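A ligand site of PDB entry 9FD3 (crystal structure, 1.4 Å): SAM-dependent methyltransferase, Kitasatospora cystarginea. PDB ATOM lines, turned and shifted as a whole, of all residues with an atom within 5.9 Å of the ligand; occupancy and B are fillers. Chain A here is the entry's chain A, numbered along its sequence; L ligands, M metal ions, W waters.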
ATOM      1  N   TYR A   4     -29.815  17.944   1.601  1.00  0.00           N
ATOM      2  CA  TYR A   4     -29.181  16.596   1.501  1.00  0.00           C
ATOM      3  C   TYR A   4     -28.616  16.202   2.867  1.00  0.00           C
ATOM      4  O   TYR A   4     -28.887  15.088   3.329  1.00  0.00           O
ATOM      5  CB  TYR A   4     -28.081  16.570   0.435  1.00  0.00           C
ATOM      6  CG  TYR A   4     -27.332  15.264   0.374  1.00  0.00           C
ATOM      7  CD1 TYR A   4     -27.736  14.240  -0.469  1.00  0.00           C
ATOM      8  CD2 TYR A   4     -26.226  15.036   1.190  1.00  0.00           C
ATOM      9  CE1 TYR A   4     -27.063  13.029  -0.517  1.00  0.00           C
ATOM     10  CE2 TYR A   4     -25.542  13.830   1.154  1.00  0.00           C
ATOM     11  CZ  TYR A   4     -25.958  12.824   0.304  1.00  0.00           C
ATOM     12  OH  TYR A   4     -25.287  11.637   0.262  1.00  0.00           O
ATOM     13  N   ARG A   8     -29.656  13.071   5.410  1.00  0.00           N
ATOM     14  CA  ARG A   8     -28.704  12.061   5.927  1.00  0.00           C
ATOM     15  C   ARG A   8     -28.899  11.929   7.450  1.00  0.00           C
ATOM     16  O   ARG A   8     -28.899  10.794   7.949  1.00  0.00           O
ATOM     17  CB  ARG A   8     -27.266  12.407   5.552  1.00  0.00           C
ATOM     18  CG  ARG A   8     -27.018  12.472   4.040  1.00  0.00           C
ATOM     19  CD  ARG A   8     -27.457  11.228   3.295  1.00  0.00           C
ATOM     20  NE  ARG A   8     -26.695  10.058   3.718  1.00  0.00           N
ATOM     21  CZ  ARG A   8     -26.938   8.808   3.327  1.00  0.00           C
ATOM     22  NH1 ARG A   8     -27.953   8.548   2.524  1.00  0.00           N
ATOM     23  NH2 ARG A   8     -26.168   7.832   3.767  1.00  0.00           N
ATOM     24  N   TYR A  19     -20.463  10.457  13.347  1.00  0.00           N
ATOM     25  CA  TYR A  19     -19.555  11.257  12.482  1.00  0.00           C
ATOM     26  C   TYR A  19     -18.643  12.094  13.398  1.00  0.00           C
ATOM     27  O   TYR A  19     -17.437  12.204  13.102  1.00  0.00           O
ATOM     28  CB  TYR A  19     -20.341  12.112  11.485  1.00  0.00           C
ATOM     29  CG  TYR A  19     -20.779  11.381  10.239  1.00  0.00           C
ATOM     30  CD1 TYR A  19     -20.184  11.619   9.014  1.00  0.00           C
ATOM     31  CD2 TYR A  19     -21.805  10.447  10.286  1.00  0.00           C
ATOM     32  CE1 TYR A  19     -20.598  10.965   7.858  1.00  0.00           C
ATOM     33  CE2 TYR A  19     -22.226   9.790   9.146  1.00  0.00           C
ATOM     34  CZ  TYR A  19     -21.624  10.039   7.926  1.00  0.00           C
ATOM     35  OH  TYR A  19     -22.068   9.392   6.811  1.00  0.00           O
ATOM     36  N   ASP A  38     -10.331  10.197   2.351  1.00  0.00           N
ATOM     37  CA  ASP A  38     -11.766   9.872   2.594  1.00  0.00           C
ATOM     38  C   ASP A  38     -12.199   8.894   1.499  1.00  0.00           C
ATOM     39  O   ASP A  38     -12.373   9.334   0.343  1.00  0.00           O
ATOM     40  CB  ASP A  38     -12.617  11.142   2.641  1.00  0.00           C
ATOM     41  CG  ASP A  38     -14.063  10.914   3.029  1.00  0.00           C
ATOM     42  OD1 ASP A  38     -14.394   9.768   3.360  1.00  0.00           O
ATOM     43  OD2 ASP A  38     -14.854  11.877   3.005  1.00  0.00           O
ATOM     44  N   LEU A  39     -12.342   7.620   1.857  1.00  0.00           N
ATOM     45  CA  LEU A  39     -12.594   6.499   0.914  1.00  0.00           C
ATOM     46  C   LEU A  39     -14.110   6.324   0.747  1.00  0.00           C
ATOM     47  O   LEU A  39     -14.808   6.153   1.761  1.00  0.00           O
ATOM     48  CB  LEU A  39     -11.957   5.252   1.512  1.00  0.00           C
ATOM     49  CG  LEU A  39     -11.763   4.065   0.577  1.00  0.00           C
ATOM     50  CD1 LEU A  39     -10.914   4.444  -0.629  1.00  0.00           C
ATOM     51  CD2 LEU A  39     -11.122   2.916   1.339  1.00  0.00           C
ATOM     52  N   GLY A  40     -14.616   6.373  -0.484  1.00  0.00           N
ATOM     53  CA  GLY A  40     -16.076   6.372  -0.728  1.00  0.00           C
ATOM     54  C   GLY A  40     -16.712   7.652  -0.209  1.00  0.00           C
ATOM     55  O   GLY A  40     -17.786   7.597   0.418  1.00  0.00           O
ATOM     56  N   ALA A  41     -16.047   8.788  -0.466  1.00  0.00           N
ATOM     57  CA  ALA A  41     -16.363  10.116   0.111  1.00  0.00           C
ATOM     58  C   ALA A  41     -17.765  10.579  -0.272  1.00  0.00           C
ATOM     59  O   ALA A  41     -18.292  11.452   0.429  1.00  0.00           O
ATOM     60  CB  ALA A  41     -15.341  11.122  -0.360  1.00  0.00           C
ATOM     61  N   GLY A  42     -18.337  10.094  -1.370  1.00  0.00           N
ATOM     62  CA  GLY A  42     -19.666  10.561  -1.833  1.00  0.00           C
ATOM     63  C   GLY A  42     -19.666  12.066  -2.018  1.00  0.00           C
ATOM     64  O   GLY A  42     -18.787  12.568  -2.749  1.00  0.00           O
ATOM     65  N   THR A  43     -20.598  12.776  -1.378  1.00  0.00           N
ATOM     66  CA  THR A  43     -20.725  14.254  -1.464  1.00  0.00           C
ATOM     67  C   THR A  43     -19.684  14.947  -0.568  1.00  0.00           C
ATOM     68  O   THR A  43     -19.679  16.188  -0.542  1.00  0.00           O
ATOM     69  CB  THR A  43     -22.129  14.732  -1.083  1.00  0.00           C
ATOM     70  OG1 THR A  43     -22.293  14.564   0.329  1.00  0.00           O
ATOM     71  CG2 THR A  43     -23.219  14.017  -1.845  1.00  0.00           C
ATOM     72  N   GLY A  44     -18.859  14.177   0.162  1.00  0.00           N
ATOM     73  CA  GLY A  44     -17.745  14.709   0.965  1.00  0.00           C
ATOM     74  C   GLY A  44     -18.150  15.071   2.389  1.00  0.00           C
ATOM     75  O   GLY A  44     -17.446  15.866   3.023  1.00  0.00           O
ATOM     76  N   LEU A  45     -19.231  14.480   2.900  1.00  0.00           N
ATOM     77  CA  LEU A  45     -19.802  14.805   4.236  1.00  0.00           C
ATOM     78  C   LEU A  45     -18.773  14.549   5.350  1.00  0.00           C
ATOM     79  O   LEU A  45     -18.609  15.440   6.200  1.00  0.00           O
ATOM     80  CB  LEU A  45     -21.064  13.967   4.427  1.00  0.00           C
ATOM     81  CG  LEU A  45     -22.032  14.416   5.502  1.00  0.00           C
ATOM     82  CD1 LEU A  45     -22.332  15.907   5.418  1.00  0.00           C
ATOM     83  CD2 LEU A  45     -23.320  13.619   5.390  1.00  0.00           C
ATOM     84  N   LEU A  46     -18.097  13.396   5.361  1.00  0.00           N
ATOM     85  CA  LEU A  46     -17.120  13.094   6.446  1.00  0.00           C
ATOM     86  C   LEU A  46     -15.896  13.999   6.263  1.00  0.00           C
ATOM     87  O   LEU A  46     -15.425  14.558   7.273  1.00  0.00           O
ATOM     88  CB  LEU A  46     -16.738  11.612   6.449  1.00  0.00           C
ATOM     89  CG  LEU A  46     -15.731  11.196   7.524  1.00  0.00           C
ATOM     90  CD1 LEU A  46     -16.178  11.633   8.906  1.00  0.00           C
ATOM     91  CD2 LEU A  46     -15.487   9.691   7.489  1.00  0.00           C
ATOM     92  N   GLN A  62     -12.042  10.295  -2.406  1.00  0.00           N
ATOM     93  CA  GLN A  62     -12.025   9.244  -3.442  1.00  0.00           C
ATOM     94  C   GLN A  62     -13.390   8.548  -3.475  1.00  0.00           C
ATOM     95  O   GLN A  62     -13.948   8.245  -2.403  1.00  0.00           O
ATOM     96  CB  GLN A  62     -10.904   8.241  -3.189  1.00  0.00           C
ATOM     97  CG  GLN A  62     -10.858   7.141  -4.226  1.00  0.00           C
ATOM     98  CD  GLN A  62      -9.618   6.301  -4.060  1.00  0.00           C
ATOM     99  OE1 GLN A  62      -8.501   6.790  -4.236  1.00  0.00           O
ATOM    100  NE2 GLN A  62      -9.808   5.025  -3.758  1.00  0.00           N
ATOM    101  N   ASP A  63     -13.903   8.304  -4.671  1.00  0.00           N
ATOM    102  CA  ASP A  63     -15.183   7.579  -4.863  1.00  0.00           C
ATOM    103  C   ASP A  63     -15.173   7.008  -6.273  1.00  0.00           C
ATOM    104  O   ASP A  63     -14.455   7.556  -7.115  1.00  0.00           O
ATOM    105  CB  ASP A  63     -16.368   8.510  -4.628  1.00  0.00           C
ATOM    106  CG  ASP A  63     -17.660   7.798  -4.255  1.00  0.00           C
ATOM    107  OD1 ASP A  63     -17.991   7.806  -3.051  1.00  0.00           O
ATOM    108  OD2 ASP A  63     -18.321   7.256  -5.172  1.00  0.00           O
ATOM    109  N   ARG A  64     -15.977   5.991  -6.542  1.00  0.00           N
ATOM    110  CA  ARG A  64     -16.116   5.480  -7.930  1.00  0.00           C
ATOM    111  C   ARG A  64     -17.115   6.345  -8.707  1.00  0.00           C
ATOM    112  O   ARG A  64     -17.069   6.284  -9.938  1.00  0.00           O
ATOM    113  CB  ARG A  64     -16.500   4.006  -7.927  1.00  0.00           C
ATOM    114  CG  ARG A  64     -17.934   3.718  -7.493  1.00  0.00           C
ATOM    115  CD  ARG A  64     -18.190   2.261  -7.805  1.00  0.00           C
ATOM    116  NE  ARG A  64     -19.393   1.753  -7.200  1.00  0.00           N
ATOM    117  CZ  ARG A  64     -19.708   0.466  -7.097  1.00  0.00           C
ATOM    118  NH1 ARG A  64     -18.881  -0.457  -7.568  1.00  0.00           N
ATOM    119  NH2 ARG A  64     -20.831   0.095  -6.512  1.00  0.00           N
ATOM    120  N   SER A  65     -17.965   7.127  -8.038  1.00  0.00           N
ATOM    121  CA  SER A  65     -19.072   7.884  -8.691  1.00  0.00           C
ATOM    122  C   SER A  65     -18.666   9.335  -8.948  1.00  0.00           C
ATOM    123  O   SER A  65     -18.567  10.120  -7.990  1.00  0.00           O
ATOM    124  CB  SER A  65     -20.334   7.821  -7.876  1.00  0.00           C
ATOM    125  OG  SER A  65     -21.316   8.698  -8.404  1.00  0.00           O
ATOM    126  N   MET A  68     -21.513  11.633  -7.561  1.00  0.00           N
ATOM    127  CA  MET A  68     -21.387  11.931  -6.116  1.00  0.00           C
ATOM    128  C   MET A  68     -20.274  12.959  -5.913  1.00  0.00           C
ATOM    129  O   MET A  68     -20.480  13.947  -5.175  1.00  0.00           O
ATOM    130  CB  MET A  68     -21.105  10.667  -5.305  1.00  0.00           C
ATOM    131  CG  MET A  68     -22.245   9.667  -5.303  1.00  0.00           C
ATOM    132  SD  MET A  68     -23.751  10.281  -4.473  1.00  0.00           S
ATOM    133  CE  MET A  68     -23.213  10.191  -2.768  1.00  0.00           C
ATOM    134  N   ALA A  87     -11.912   6.445  -8.270  1.00  0.00           N
ATOM    135  CA  ALA A  87     -11.395   5.065  -8.193  1.00  0.00           C
ATOM    136  C   ALA A  87     -12.360   4.200  -7.384  1.00  0.00           C
ATOM    137  O   ALA A  87     -12.962   4.694  -6.404  1.00  0.00           O
ATOM    138  CB  ALA A  87     -10.012   5.046  -7.586  1.00  0.00           C
ATOM    139  N   ASP A  88     -12.469   2.938  -7.792  1.00  0.00           N
ATOM    140  CA  ASP A  88     -13.189   1.906  -7.015  1.00  0.00           C
ATOM    141  C   ASP A  88     -12.322   1.545  -5.796  1.00  0.00           C
ATOM    142  O   ASP A  88     -11.078   1.607  -5.906  1.00  0.00           O
ATOM    143  CB  ASP A  88     -13.490   0.697  -7.890  1.00  0.00           C
ATOM    144  CG  ASP A  88     -14.602  -0.167  -7.342  1.00  0.00           C
ATOM    145  OD1 ASP A  88     -15.712  -0.102  -7.889  1.00  0.00           O
ATOM    146  OD2 ASP A  88     -14.348  -0.892  -6.357  1.00  0.00           O
ATOM    147  N   HIS A  89     -12.935   1.151  -4.683  1.00  0.00           N
ATOM    148  CA  HIS A  89     -12.199   0.558  -3.541  1.00  0.00           C
ATOM    149  C   HIS A  89     -11.277  -0.571  -4.026  1.00  0.00           C
ATOM    150  O   HIS A  89     -10.232  -0.773  -3.397  1.00  0.00           O
ATOM    151  CB  HIS A  89     -13.150   0.008  -2.489  1.00  0.00           C
ATOM    152  CG  HIS A  89     -14.103   1.002  -1.928  1.00  0.00           C
ATOM    153  ND1 HIS A  89     -13.808   2.339  -1.843  1.00  0.00           N
ATOM    154  CD2 HIS A  89     -15.342   0.844  -1.397  1.00  0.00           C
ATOM    155  CE1 HIS A  89     -14.836   2.970  -1.301  1.00  0.00           C
ATOM    156  NE2 HIS A  89     -15.787   2.067  -1.018  1.00  0.00           N
ATOM    157  N   LEU A  90     -11.694  -1.311  -5.059  1.00  0.00           N
ATOM    158  CA  LEU A  90     -10.965  -2.512  -5.537  1.00  0.00           C
ATOM    159  C   LEU A  90      -9.755  -2.101  -6.402  1.00  0.00           C
ATOM    160  O   LEU A  90      -8.889  -2.957  -6.641  1.00  0.00           O
ATOM    161  CB  LEU A  90     -11.931  -3.409  -6.329  1.00  0.00           C
ATOM    162  CG  LEU A  90     -13.096  -3.957  -5.517  1.00  0.00           C
ATOM    163  CD1 LEU A  90     -13.990  -4.825  -6.383  1.00  0.00           C
ATOM    164  CD2 LEU A  90     -12.602  -4.735  -4.306  1.00  0.00           C
ATOM    165  N   SER A 103     -13.614   6.487   6.281  1.00  0.00           N
ATOM    166  CA  SER A 103     -14.699   6.048   5.384  1.00  0.00           C
ATOM    167  C   SER A 103     -16.016   6.117   6.154  1.00  0.00           C
ATOM    168  O   SER A 103     -15.999   5.822   7.362  1.00  0.00           O
ATOM    169  CB  SER A 103     -14.416   4.675   4.854  1.00  0.00           C
ATOM    170  OG  SER A 103     -15.289   4.365   3.775  1.00  0.00           O
ATOM    171  N   ALA A 104     -17.093   6.499   5.486  1.00  0.00           N
ATOM    172  CA  ALA A 104     -18.452   6.465   6.071  1.00  0.00           C
ATOM    173  C   ALA A 104     -19.423   5.817   5.085  1.00  0.00           C
ATOM    174  O   ALA A 104     -19.550   6.308   3.952  1.00  0.00           O
ATOM    175  CB  ALA A 104     -18.900   7.842   6.473  1.00  0.00           C
ATOM    176  N   LEU A 105     -20.062   4.733   5.527  1.00  0.00           N
ATOM    177  CA  LEU A 105     -21.232   4.082   4.889  1.00  0.00           C
ATOM    178  C   LEU A 105     -20.905   3.683   3.447  1.00  0.00           C
ATOM    179  O   LEU A 105     -21.766   3.835   2.570  1.00  0.00           O
ATOM    180  CB  LEU A 105     -22.435   5.038   4.966  1.00  0.00           C
ATOM    181  CG  LEU A 105     -22.838   5.435   6.386  1.00  0.00           C
ATOM    182  CD1 LEU A 105     -24.009   6.412   6.354  1.00  0.00           C
ATOM    183  CD2 LEU A 105     -23.189   4.201   7.206  1.00  0.00           C
ATOM    184  N   SER A 106     -19.706   3.130   3.212  1.00  0.00           N
ATOM    185  CA  SER A 106     -19.239   2.786   1.846  1.00  0.00           C
ATOM    186  C   SER A 106     -18.697   1.360   1.763  1.00  0.00           C
ATOM    187  O   SER A 106     -18.979   0.673   0.780  1.00  0.00           O
ATOM    188  CB  SER A 106     -18.219   3.800   1.382  1.00  0.00           C
ATOM    189  OG  SER A 106     -17.885   3.583   0.023  1.00  0.00           O
ATOM    190  N   HIS A 109     -20.446  -2.022   0.815  1.00  0.00           N
ATOM    191  CA  HIS A 109     -20.809  -2.328  -0.599  1.00  0.00           C
ATOM    192  C   HIS A 109     -19.871  -3.388  -1.187  1.00  0.00           C
ATOM    193  O   HIS A 109     -20.138  -3.824  -2.333  1.00  0.00           O
ATOM    194  CB  HIS A 109     -20.820  -1.060  -1.455  1.00  0.00           C
ATOM    195  CG  HIS A 109     -21.990  -0.179  -1.182  1.00  0.00           C
ATOM    196  ND1 HIS A 109     -23.253  -0.486  -1.653  1.00  0.00           N
ATOM    197  CD2 HIS A 109     -22.103   0.970  -0.498  1.00  0.00           C
ATOM    198  CE1 HIS A 109     -24.093   0.447  -1.266  1.00  0.00           C
ATOM    199  NE2 HIS A 109     -23.415   1.356  -0.552  1.00  0.00           N
ATOM    200  N   LEU A 110     -18.822  -3.796  -0.461  1.00  0.00           N
ATOM    201  CA  LEU A 110     -17.862  -4.837  -0.917  1.00  0.00           C
ATOM    202  C   LEU A 110     -18.226  -6.205  -0.329  1.00  0.00           C
ATOM    203  O   LEU A 110     -18.742  -6.255   0.799  1.00  0.00           O
ATOM    204  CB  LEU A 110     -16.444  -4.463  -0.475  1.00  0.00           C
ATOM    205  CG  LEU A 110     -15.897  -3.128  -0.973  1.00  0.00           C
ATOM    206  CD1 LEU A 110     -14.500  -2.917  -0.425  1.00  0.00           C
ATOM    207  CD2 LEU A 110     -15.888  -3.041  -2.485  1.00  0.00           C
HETATM  208  N1  LIG L   1     -19.126   8.803   2.651  1.00  0.00           N
HETATM  209  C1  LIG L   1     -20.310   9.560   2.172  1.00  0.00           C
HETATM  210  C2  LIG L   1     -21.123   8.751   1.148  1.00  0.00           C
HETATM  211  C3  LIG L   1     -21.745   7.462   1.649  1.00  0.00           C
HETATM  212  S1  LIG L   1     -22.842   6.704   0.414  1.00  0.00           S
HETATM  213  C4  LIG L   1     -21.173   9.961   3.368  1.00  0.00           C
HETATM  214  O1  LIG L   1     -20.829   9.622   4.497  1.00  0.00           O
HETATM  215  O2  LIG L   1     -22.196  10.627   3.184  1.00  0.00           O
HETATM  216  C5  LIG L   1     -21.800   5.388  -0.279  1.00  0.00           C
HETATM  217  C6  LIG L   1     -20.726   5.877  -1.220  1.00  0.00           C
HETATM  218  O3  LIG L   1     -19.877   4.758  -1.540  1.00  0.00           O
HETATM  219  C7  LIG L   1     -21.237   6.434  -2.553  1.00  0.00           C
HETATM  220  O4  LIG L   1     -20.674   7.715  -2.824  1.00  0.00           O
HETATM  221  C8  LIG L   1     -20.840   5.352  -3.564  1.00  0.00           C
HETATM  222  O5  LIG L   1     -20.590   5.839  -4.869  1.00  0.00           O
HETATM  223  C9  LIG L   1     -19.571   4.821  -2.918  1.00  0.00           C
HETATM  224  N2  LIG L   1     -19.172   3.481  -3.329  1.00  0.00           N
HETATM  225  C10 LIG L   1     -19.924   2.331  -3.272  1.00  0.00           C
HETATM  226  N3  LIG L   1     -19.272   1.271  -3.669  1.00  0.00           N
HETATM  227  C11 LIG L   1     -18.013   1.740  -3.992  1.00  0.00           C
HETATM  228  C12 LIG L   1     -16.856   1.095  -4.478  1.00  0.00           C
HETATM  229  N4  LIG L   1     -16.786  -0.214  -4.699  1.00  0.00           N
HETATM  230  N5  LIG L   1     -15.760   1.860  -4.696  1.00  0.00           N
HETATM  231  C13 LIG L   1     -15.838   3.171  -4.452  1.00  0.00           C
HETATM  232  N6  LIG L   1     -16.866   3.885  -4.004  1.00  0.00           N
HETATM  233  C14 LIG L   1     -17.932   3.105  -3.790  1.00  0.00           C
HETATM  234 CA    CA M   1     -25.128   1.750   1.385  1.00  0.00          CA
HETATM  235  O   HOH W   1     -21.457   4.218  -6.979  1.00  0.00           O
HETATM  236  O   HOH W   2     -24.132   9.924   4.943  1.00  0.00           O
HETATM  237  O   HOH W   3     -18.921  -2.120  -4.652  1.00  0.00           O
HETATM  238  O   HOH W   4     -16.423   8.077   3.151  1.00  0.00           O
HETATM  239  O   HOH W   5     -17.624  11.391   3.183  1.00  0.00           O
HETATM  240  O   HOH W   6     -22.624  11.896   0.804  1.00  0.00           O
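Water W2 lies within hydrogen-bond range of O2 of the ligand (2.7 Å), OH of Tyr 19 (2.8 Å) and NE of Arg 8 (2.8 Å).
Water W6 lies within hydrogen-bond range of OH of Tyr 4, OG1 of Thr 43 and O2 of the ligand.
Water W1 bridges O5 of the ligand and NE of Arg 64.
Water W3 lies within hydrogen-bond range of a nitrogen (N4) of the ligand, the backbone carbonyl oxygen of His 109 and the guanidinium group of Arg 64.
Water W5 lies within hydrogen-bond range of OD2 of Asp 38 (2.8 Å), O of Ala 41 (2.8 Å), N of Leu 46 (3.0 Å), N1 of the ligand (3.0 Å) and N of Leu 45 (3.5 Å).
A sulfur (S1) of the ligand sits close to the backbone carbonyl oxygen (O) of Leu 105 (3.7 Å).
Residues that only touch the ligand: Ala 41, Gly 42, Leu 45, Ser 65, Met 68, Ala 87, His 109 and Leu 110.
Hydrophobic or aromatic side chains within 4 Å of the ligand: Tyr 19, Leu 45, Met 68, His 89, Ala 104, His 109 and Leu 110.
Within 4 Å of the ligand: Tyr 19, Gly 40, Ala 41, Gly 42, Leu 45, Asp 63, Arg 64, Ser 65, Met 68, Ala 87, Asp 88, His 89, Ala 104, Leu 105, Ser 106, His 109 and Leu 110.
The nearest printed residue that does not touch the ligand is Tyr 4 (4.4 Å).
The side-chain hydroxyl (OG) of Ser 106 is in hydrogen-bond range of an oxygen (O3) of the ligand.
The side-chain hydroxyl of Tyr 19 lies within hydrogen-bond range of an oxygen (O1) of the ligand (2.6 Å).
The side-chain carboxylate (OD2) of Asp 88 is in hydrogen-bond range of a nitrogen (N4) of the ligand.
The backbone NH (N) of His 89 sits at hydrogen-bond distance from a nitrogen (N5) of the ligand (2.9 Å).
O of Ala 104 sits at hydrogen-bond distance from N1 of the ligand (2.8 Å).
The backbone NH (N) of Arg 64 is in hydrogen-bond range of a nitrogen (N6) of the ligand, 3.4 Å away.
N1 of the ligand sits at hydrogen-bond distance from O of Gly 40.
OD2 of Asp 63 is in hydrogen-bond range of O5 of the ligand.
A nitrogen (N5) of the ligand sits close to a ring nitrogen (ND1) of His 89 (3.5 Å).
N3 of the ligand is in hydrogen-bond range of NH2 of Arg 64 (3.4 Å).
OD1 of Asp 88 is in salt-bridge range of NH1 of Arg 64, at 3.2 Å.
N of Gly 40 sits at hydrogen-bond distance from O of Gln 62 (2.8 Å).
The backbone carbonyl oxygen (O) of Asp 63 sits at hydrogen-bond distance from the backbone NH (N) of Ala 87 (3.0 Å).
OD2 of Asp 63 lies within hydrogen-bond range of N of Ser 65, 2.9 Å away.
The backbone NH of Met 68 lies within hydrogen-bond range of the side-chain hydroxyl of Ser 65 (3.1 Å).
The side-chain carboxylate of Asp 63 is in hydrogen-bond range of the backbone NH of Gly 42.
The side-chain hydroxyl (OG) of Ser 106 sits at hydrogen-bond distance from a ring nitrogen (NE2) of His 89 (2.8 Å).
The backbone carbonyl oxygen (O) of Gln 62 is in hydrogen-bond range of the backbone NH (N) of Ala 41.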
